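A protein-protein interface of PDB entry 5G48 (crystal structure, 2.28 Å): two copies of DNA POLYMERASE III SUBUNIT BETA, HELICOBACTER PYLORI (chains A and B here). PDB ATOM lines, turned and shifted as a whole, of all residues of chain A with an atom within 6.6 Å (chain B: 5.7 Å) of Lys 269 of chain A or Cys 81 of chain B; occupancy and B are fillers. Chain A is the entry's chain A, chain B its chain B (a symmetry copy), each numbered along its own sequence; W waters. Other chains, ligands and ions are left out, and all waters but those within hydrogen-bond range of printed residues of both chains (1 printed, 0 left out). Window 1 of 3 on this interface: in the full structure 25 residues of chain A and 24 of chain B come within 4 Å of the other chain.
Of chain B, only Cys 81 comes within 4 Å of Lys 269 of chain A.
Cys 81 of chain B touches just these residues of chain A: Lys 269 and Leu 270.
Of the printed residues of chain B, Leu 270 of chain A touches Cys 81 and Leu 82.
Of the printed residues of chain B, Glu 266 of chain A touches Lys 83.
Printed residues of chain A within 4 Å of Lys 83 of chain B: Glu 266.
The nearest printed residue of chain A that does not touch Lys 83 of chain B is Leu 270 of chain A (6.7 Å).
The side-chain carboxylate (OE1) of Glu 266 of chain A lies within salt-bridge range of the side-chain amino group (NZ) of Lys 83 of chain B (3.6 Å).
Among the printed residues, pairs that only touch across the chains: Ser 273 of chain A with Ile 78 of chain B (3.6 Å), Leu 270 of chain A with Leu 82 of chain B (3.7 Å), Lys 269 of chain A with Cys 81 of chain B (3.8 Å) and Leu 270 of chain A with Cys 81 of chain B (3.9 Å).
Water W1 bridges the backbone carbonyl oxygen of Cys 81 of chain B (2.9 Å) and the backbone carbonyl oxygen of Glu 266 of chain A (3.0 Å).
Along chain B the printed residues that touch a printed residue of chain A span positions 78 to 83.
Among the printed residues, 5 pairs touch across the chains.
Among the printed residues, Asp or Glu carboxylates within 4 Å of a Lys or Arg side-chain nitrogen of the other chain: Glu 266 of chain A with Lys 83 of chain B.
No position is printed for both chains.
The backbone carbonyl oxygen (O) of Lys 269 of chain A sits at hydrogen-bond distance from the side-chain hydroxyl (OG) of Ser 272 of chain A (2.7 Å).
The side-chain sulfur (SG) of Cys 81 of chain B lies within hydrogen-bond range of the backbone carbonyl oxygen (O) of Asp 77 of chain B.
The backbone carbonyl oxygen of Leu 270 of chain A lies within hydrogen-bond range of the side-chain hydroxyl of Ser 273 of chain A (2.7 Å).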
ATOM      1  N   PHE A 264     -21.759  24.371  11.117  1.00  0.00           N
ATOM      2  CA  PHE A 264     -20.561  23.532  11.232  1.00  0.00           C
ATOM      3  C   PHE A 264     -19.282  24.372  11.311  1.00  0.00           C
ATOM      4  O   PHE A 264     -18.395  24.062  12.109  1.00  0.00           O
ATOM      5  CB  PHE A 264     -20.482  22.491  10.100  1.00  0.00           C
ATOM      6  CG  PHE A 264     -21.108  21.163  10.459  1.00  0.00           C
ATOM      7  CD1 PHE A 264     -22.485  21.054  10.636  1.00  0.00           C
ATOM      8  CD2 PHE A 264     -20.323  20.029  10.640  1.00  0.00           C
ATOM      9  CE1 PHE A 264     -23.067  19.841  10.982  1.00  0.00           C
ATOM     10  CE2 PHE A 264     -20.901  18.815  10.976  1.00  0.00           C
ATOM     11  CZ  PHE A 264     -22.275  18.721  11.156  1.00  0.00           C
ATOM     12  N   LYS A 265     -19.197  25.423  10.493  1.00  0.00           N
ATOM     13  CA  LYS A 265     -18.089  26.378  10.577  1.00  0.00           C
ATOM     14  C   LYS A 265     -17.933  26.925  11.990  1.00  0.00           C
ATOM     15  O   LYS A 265     -16.848  26.862  12.551  1.00  0.00           O
ATOM     16  CB  LYS A 265     -18.276  27.559   9.620  1.00  0.00           C
ATOM     17  CG  LYS A 265     -17.906  27.287   8.180  1.00  0.00           C
ATOM     18  CD  LYS A 265     -17.881  28.596   7.412  1.00  0.00           C
ATOM     19  CE  LYS A 265     -17.884  28.378   5.913  1.00  0.00           C
ATOM     20  NZ  LYS A 265     -17.743  29.681   5.202  1.00  0.00           N
ATOM     21  N   GLU A 266     -19.029  27.444  12.542  1.00  0.00           N
ATOM     22  CA  GLU A 266     -19.056  28.023  13.891  1.00  0.00           C
ATOM     23  C   GLU A 266     -18.670  27.032  14.987  1.00  0.00           C
ATOM     24  O   GLU A 266     -17.930  27.380  15.906  1.00  0.00           O
ATOM     25  CB  GLU A 266     -20.451  28.569  14.215  1.00  0.00           C
ATOM     26  CG  GLU A 266     -20.851  29.819  13.436  1.00  0.00           C
ATOM     27  CD  GLU A 266     -22.263  30.287  13.760  1.00  0.00           C
ATOM     28  OE1 GLU A 266     -22.918  29.689  14.641  1.00  0.00           O
ATOM     29  OE2 GLU A 266     -22.724  31.267  13.140  1.00  0.00           O
ATOM     30  N   SER A 267     -19.185  25.809  14.892  1.00  0.00           N
ATOM     31  CA  SER A 267     -18.948  24.788  15.912  1.00  0.00           C
ATOM     32  C   SER A 267     -17.508  24.268  15.886  1.00  0.00           C
ATOM     33  O   SER A 267     -16.906  24.016  16.938  1.00  0.00           O
ATOM     34  CB  SER A 267     -19.922  23.630  15.734  1.00  0.00           C
ATOM     35  OG  SER A 267     -21.262  24.091  15.759  1.00  0.00           O
ATOM     36  N   ILE A 268     -16.969  24.108  14.683  1.00  0.00           N
ATOM     37  CA  ILE A 268     -15.583  23.678  14.500  1.00  0.00           C
ATOM     38  C   ILE A 268     -14.600  24.770  14.929  1.00  0.00           C
ATOM     39  O   ILE A 268     -13.639  24.485  15.640  1.00  0.00           O
ATOM     40  CB  ILE A 268     -15.333  23.231  13.041  1.00  0.00           C
ATOM     41  CG1 ILE A 268     -16.019  21.879  12.806  1.00  0.00           C
ATOM     42  CG2 ILE A 268     -13.841  23.139  12.727  1.00  0.00           C
ATOM     43  CD1 ILE A 268     -16.331  21.578  11.358  1.00  0.00           C
ATOM     44  N   LYS A 269     -14.845  26.001  14.479  1.00  0.00           N
ATOM     45  CA  LYS A 269     -14.072  27.176  14.918  1.00  0.00           C
ATOM     46  C   LYS A 269     -14.039  27.260  16.449  1.00  0.00           C
ATOM     47  O   LYS A 269     -12.986  27.460  17.045  1.00  0.00           O
ATOM     48  CB  LYS A 269     -14.661  28.477  14.338  1.00  0.00           C
ATOM     49  CG  LYS A 269     -13.638  29.423  13.718  1.00  0.00           C
ATOM     50  CD  LYS A 269     -14.296  30.438  12.783  1.00  0.00           C
ATOM     51  CE  LYS A 269     -14.562  29.864  11.394  1.00  0.00           C
ATOM     52  NZ  LYS A 269     -14.781  30.919  10.358  1.00  0.00           N
ATOM     53  N   LEU A 270     -15.206  27.081  17.061  1.00  0.00           N
ATOM     54  CA  LEU A 270     -15.363  27.135  18.512  1.00  0.00           C
ATOM     55  C   LEU A 270     -14.522  26.071  19.218  1.00  0.00           C
ATOM     56  O   LEU A 270     -13.769  26.391  20.141  1.00  0.00           O
ATOM     57  CB  LEU A 270     -16.848  26.993  18.878  1.00  0.00           C
ATOM     58  CG  LEU A 270     -17.277  27.012  20.348  1.00  0.00           C
ATOM     59  CD1 LEU A 270     -18.673  27.611  20.485  1.00  0.00           C
ATOM     60  CD2 LEU A 270     -17.222  25.626  20.991  1.00  0.00           C
ATOM     61  N   CYS A 271     -14.647  24.820  18.778  1.00  0.00           N
ATOM     62  CA  CYS A 271     -13.867  23.717  19.358  1.00  0.00           C
ATOM     63  C   CYS A 271     -12.370  23.816  19.075  1.00  0.00           C
ATOM     64  O   CYS A 271     -11.560  23.340  19.872  1.00  0.00           O
ATOM     65  CB  CYS A 271     -14.395  22.358  18.891  1.00  0.00           C
ATOM     66  SG  CYS A 271     -15.979  21.921  19.635  1.00  0.00           S
ATOM     67  N   SER A 272     -12.003  24.429  17.954  1.00  0.00           N
ATOM     68  CA  SER A 272     -10.595  24.584  17.588  1.00  0.00           C
ATOM     69  C   SER A 272      -9.857  25.665  18.399  1.00  0.00           C
ATOM     70  O   SER A 272      -8.649  25.836  18.225  1.00  0.00           O
ATOM     71  CB  SER A 272     -10.446  24.850  16.086  1.00  0.00           C
ATOM     72  OG  SER A 272     -11.026  26.086  15.732  1.00  0.00           O
ATOM     73  N   SER A 273     -10.571  26.392  19.265  1.00  0.00           N
ATOM     74  CA  SER A 273      -9.942  27.265  20.265  1.00  0.00           C
ATOM     75  C   SER A 273      -8.953  26.540  21.190  1.00  0.00           C
ATOM     76  O   SER A 273      -7.992  27.152  21.648  1.00  0.00           O
ATOM     77  CB  SER A 273     -11.007  27.961  21.119  1.00  0.00           C
ATOM     78  OG  SER A 273     -11.752  27.019  21.875  1.00  0.00           O
ATOM     79  N   LEU A 274      -9.197  25.256  21.469  1.00  0.00           N
ATOM     80  CA  LEU A 274      -8.311  24.441  22.315  1.00  0.00           C
ATOM     81  C   LEU A 274      -7.621  23.264  21.623  1.00  0.00           C
ATOM     82  O   LEU A 274      -6.786  22.603  22.242  1.00  0.00           O
ATOM     83  CB  LEU A 274      -9.093  23.907  23.518  1.00  0.00           C
ATOM     84  CG  LEU A 274      -9.744  24.970  24.401  1.00  0.00           C
ATOM     85  CD1 LEU A 274     -10.537  24.295  25.509  1.00  0.00           C
ATOM     86  CD2 LEU A 274      -8.693  25.913  24.968  1.00  0.00           C
ATOM     87  N   ILE A 278     -10.743  17.535  15.960  1.00  0.00           N
ATOM     88  CA  ILE A 278     -12.081  17.540  16.554  1.00  0.00           C
ATOM     89  C   ILE A 278     -12.751  16.177  16.365  1.00  0.00           C
ATOM     90  O   ILE A 278     -12.583  15.534  15.323  1.00  0.00           O
ATOM     91  CB  ILE A 278     -12.943  18.668  15.925  1.00  0.00           C
ATOM     92  CG1 ILE A 278     -12.538  20.019  16.526  1.00  0.00           C
ATOM     93  CG2 ILE A 278     -14.443  18.442  16.142  1.00  0.00           C
ATOM     94  CD1 ILE A 278     -12.960  21.209  15.703  1.00  0.00           C
ATOM     95  N   ALA A 322      -9.577  20.200  12.128  1.00  0.00           N
ATOM     96  CA  ALA A 322     -10.487  21.353  12.172  1.00  0.00           C
ATOM     97  C   ALA A 322     -10.280  22.308  11.010  1.00  0.00           C
ATOM     98  O   ALA A 322     -11.240  22.696  10.335  1.00  0.00           O
ATOM     99  CB  ALA A 322     -10.321  22.106  13.484  1.00  0.00           C
ATOM    100  N   LEU A 326     -12.682  23.196   7.841  1.00  0.00           N
ATOM    101  CA  LEU A 326     -13.121  24.585   7.637  1.00  0.00           C
ATOM    102  C   LEU A 326     -12.843  25.084   6.224  1.00  0.00           C
ATOM    103  O   LEU A 326     -13.730  25.656   5.580  1.00  0.00           O
ATOM    104  CB  LEU A 326     -12.449  25.534   8.637  1.00  0.00           C
ATOM    105  CG  LEU A 326     -13.042  25.524  10.038  1.00  0.00           C
ATOM    106  CD1 LEU A 326     -12.099  26.199  11.026  1.00  0.00           C
ATOM    107  CD2 LEU A 326     -14.413  26.194  10.045  1.00  0.00           C
ATOM    108  N   ASN A 330     -15.241  26.428   3.457  1.00  0.00           N
ATOM    109  CA  ASN A 330     -15.002  27.755   2.843  1.00  0.00           C
ATOM    110  C   ASN A 330     -15.006  27.756   1.321  1.00  0.00           C
ATOM    111  O   ASN A 330     -15.365  28.763   0.707  1.00  0.00           O
ATOM    112  CB  ASN A 330     -13.684  28.377   3.334  1.00  0.00           C
ATOM    113  CG  ASN A 330     -13.719  28.751   4.807  1.00  0.00           C
ATOM    114  OD1 ASN A 330     -14.786  28.895   5.402  1.00  0.00           O
ATOM    115  ND2 ASN A 330     -12.541  28.904   5.406  1.00  0.00           N
ATOM    116  N   LEU B  76      -9.492  34.182  26.324  1.00  0.00           N
ATOM    117  CA  LEU B  76      -9.905  35.130  25.272  1.00  0.00           C
ATOM    118  C   LEU B  76     -10.310  34.430  23.972  1.00  0.00           C
ATOM    119  O   LEU B  76     -11.309  34.805  23.352  1.00  0.00           O
ATOM    120  CB  LEU B  76      -8.796  36.152  24.976  1.00  0.00           C
ATOM    121  CG  LEU B  76      -9.051  37.175  23.854  1.00  0.00           C
ATOM    122  CD1 LEU B  76     -10.283  38.012  24.148  1.00  0.00           C
ATOM    123  CD2 LEU B  76      -7.835  38.066  23.662  1.00  0.00           C
ATOM    124  N   ASP B  77      -9.533  33.432  23.556  1.00  0.00           N
ATOM    125  CA  ASP B  77      -9.854  32.664  22.341  1.00  0.00           C
ATOM    126  C   ASP B  77     -11.235  32.004  22.411  1.00  0.00           C
ATOM    127  O   ASP B  77     -11.997  32.056  21.441  1.00  0.00           O
ATOM    128  CB  ASP B  77      -8.788  31.601  22.067  1.00  0.00           C
ATOM    129  CG  ASP B  77      -7.454  32.194  21.633  1.00  0.00           C
ATOM    130  OD1 ASP B  77      -7.387  33.403  21.315  1.00  0.00           O
ATOM    131  OD2 ASP B  77      -6.463  31.437  21.615  1.00  0.00           O
ATOM    132  N   ILE B  78     -11.551  31.401  23.555  1.00  0.00           N
ATOM    133  CA  ILE B  78     -12.869  30.800  23.784  1.00  0.00           C
ATOM    134  C   ILE B  78     -14.002  31.836  23.711  1.00  0.00           C
ATOM    135  O   ILE B  78     -14.959  31.640  22.963  1.00  0.00           O
ATOM    136  CB  ILE B  78     -12.922  30.046  25.139  1.00  0.00           C
ATOM    137  CG1 ILE B  78     -12.079  28.761  25.058  1.00  0.00           C
ATOM    138  CG2 ILE B  78     -14.363  29.711  25.537  1.00  0.00           C
ATOM    139  CD1 ILE B  78     -11.673  28.191  26.404  1.00  0.00           C
ATOM    140  N   ILE B  79     -13.891  32.923  24.475  1.00  0.00           N
ATOM    141  CA  ILE B  79     -14.968  33.917  24.562  1.00  0.00           C
ATOM    142  C   ILE B  79     -15.232  34.588  23.207  1.00  0.00           C
ATOM    143  O   ILE B  79     -16.388  34.824  22.860  1.00  0.00           O
ATOM    144  CB  ILE B  79     -14.711  35.004  25.645  1.00  0.00           C
ATOM    145  CG1 ILE B  79     -14.478  34.386  27.037  1.00  0.00           C
ATOM    146  CG2 ILE B  79     -15.883  35.986  25.717  1.00  0.00           C
ATOM    147  CD1 ILE B  79     -15.497  33.351  27.464  1.00  0.00           C
ATOM    148  N   SER B  80     -14.177  34.855  22.434  1.00  0.00           N
ATOM    149  CA  SER B  80     -14.325  35.464  21.102  1.00  0.00           C
ATOM    150  C   SER B  80     -15.043  34.563  20.079  1.00  0.00           C
ATOM    151  O   SER B  80     -15.514  35.060  19.059  1.00  0.00           O
ATOM    152  CB  SER B  80     -12.966  35.933  20.548  1.00  0.00           C
ATOM    153  OG  SER B  80     -12.137  34.846  20.171  1.00  0.00           O
ATOM    154  N   CYS B  81     -15.127  33.258  20.358  1.00  0.00           N
ATOM    155  CA  CYS B  81     -15.900  32.309  19.537  1.00  0.00           C
ATOM    156  C   CYS B  81     -17.371  32.142  19.957  1.00  0.00           C
ATOM    157  O   CYS B  81     -18.085  31.327  19.369  1.00  0.00           O
ATOM    158  CB  CYS B  81     -15.218  30.933  19.541  1.00  0.00           C
ATOM    159  SG  CYS B  81     -13.653  30.887  18.649  1.00  0.00           S
ATOM    160  N   LEU B  82     -17.828  32.899  20.953  1.00  0.00           N
ATOM    161  CA  LEU B  82     -19.194  32.762  21.460  1.00  0.00           C
ATOM    162  C   LEU B  82     -20.121  33.892  20.993  1.00  0.00           C
ATOM    163  O   LEU B  82     -19.668  34.936  20.519  1.00  0.00           O
ATOM    164  CB  LEU B  82     -19.168  32.681  22.988  1.00  0.00           C
ATOM    165  CG  LEU B  82     -18.522  31.420  23.580  1.00  0.00           C
ATOM    166  CD1 LEU B  82     -18.446  31.523  25.097  1.00  0.00           C
ATOM    167  CD2 LEU B  82     -19.266  30.156  23.160  1.00  0.00           C
ATOM    168  N   LYS B  83     -21.425  33.651  21.128  1.00  0.00           N
ATOM    169  CA  LYS B  83     -22.466  34.631  20.789  1.00  0.00           C
ATOM    170  C   LYS B  83     -22.511  35.768  21.814  1.00  0.00           C
ATOM    171  O   LYS B  83     -21.880  35.685  22.866  1.00  0.00           O
ATOM    172  CB  LYS B  83     -23.832  33.938  20.715  1.00  0.00           C
ATOM    173  CG  LYS B  83     -23.971  32.935  19.568  1.00  0.00           C
ATOM    174  CD  LYS B  83     -24.701  31.662  20.000  1.00  0.00           C
ATOM    175  CE  LYS B  83     -25.444  30.987  18.853  1.00  0.00           C
ATOM    176  NZ  LYS B  83     -24.608  30.778  17.637  1.00  0.00           N
HETATM  177  O   HOH W   1     -17.260  30.131  16.813  1.00  0.00           O
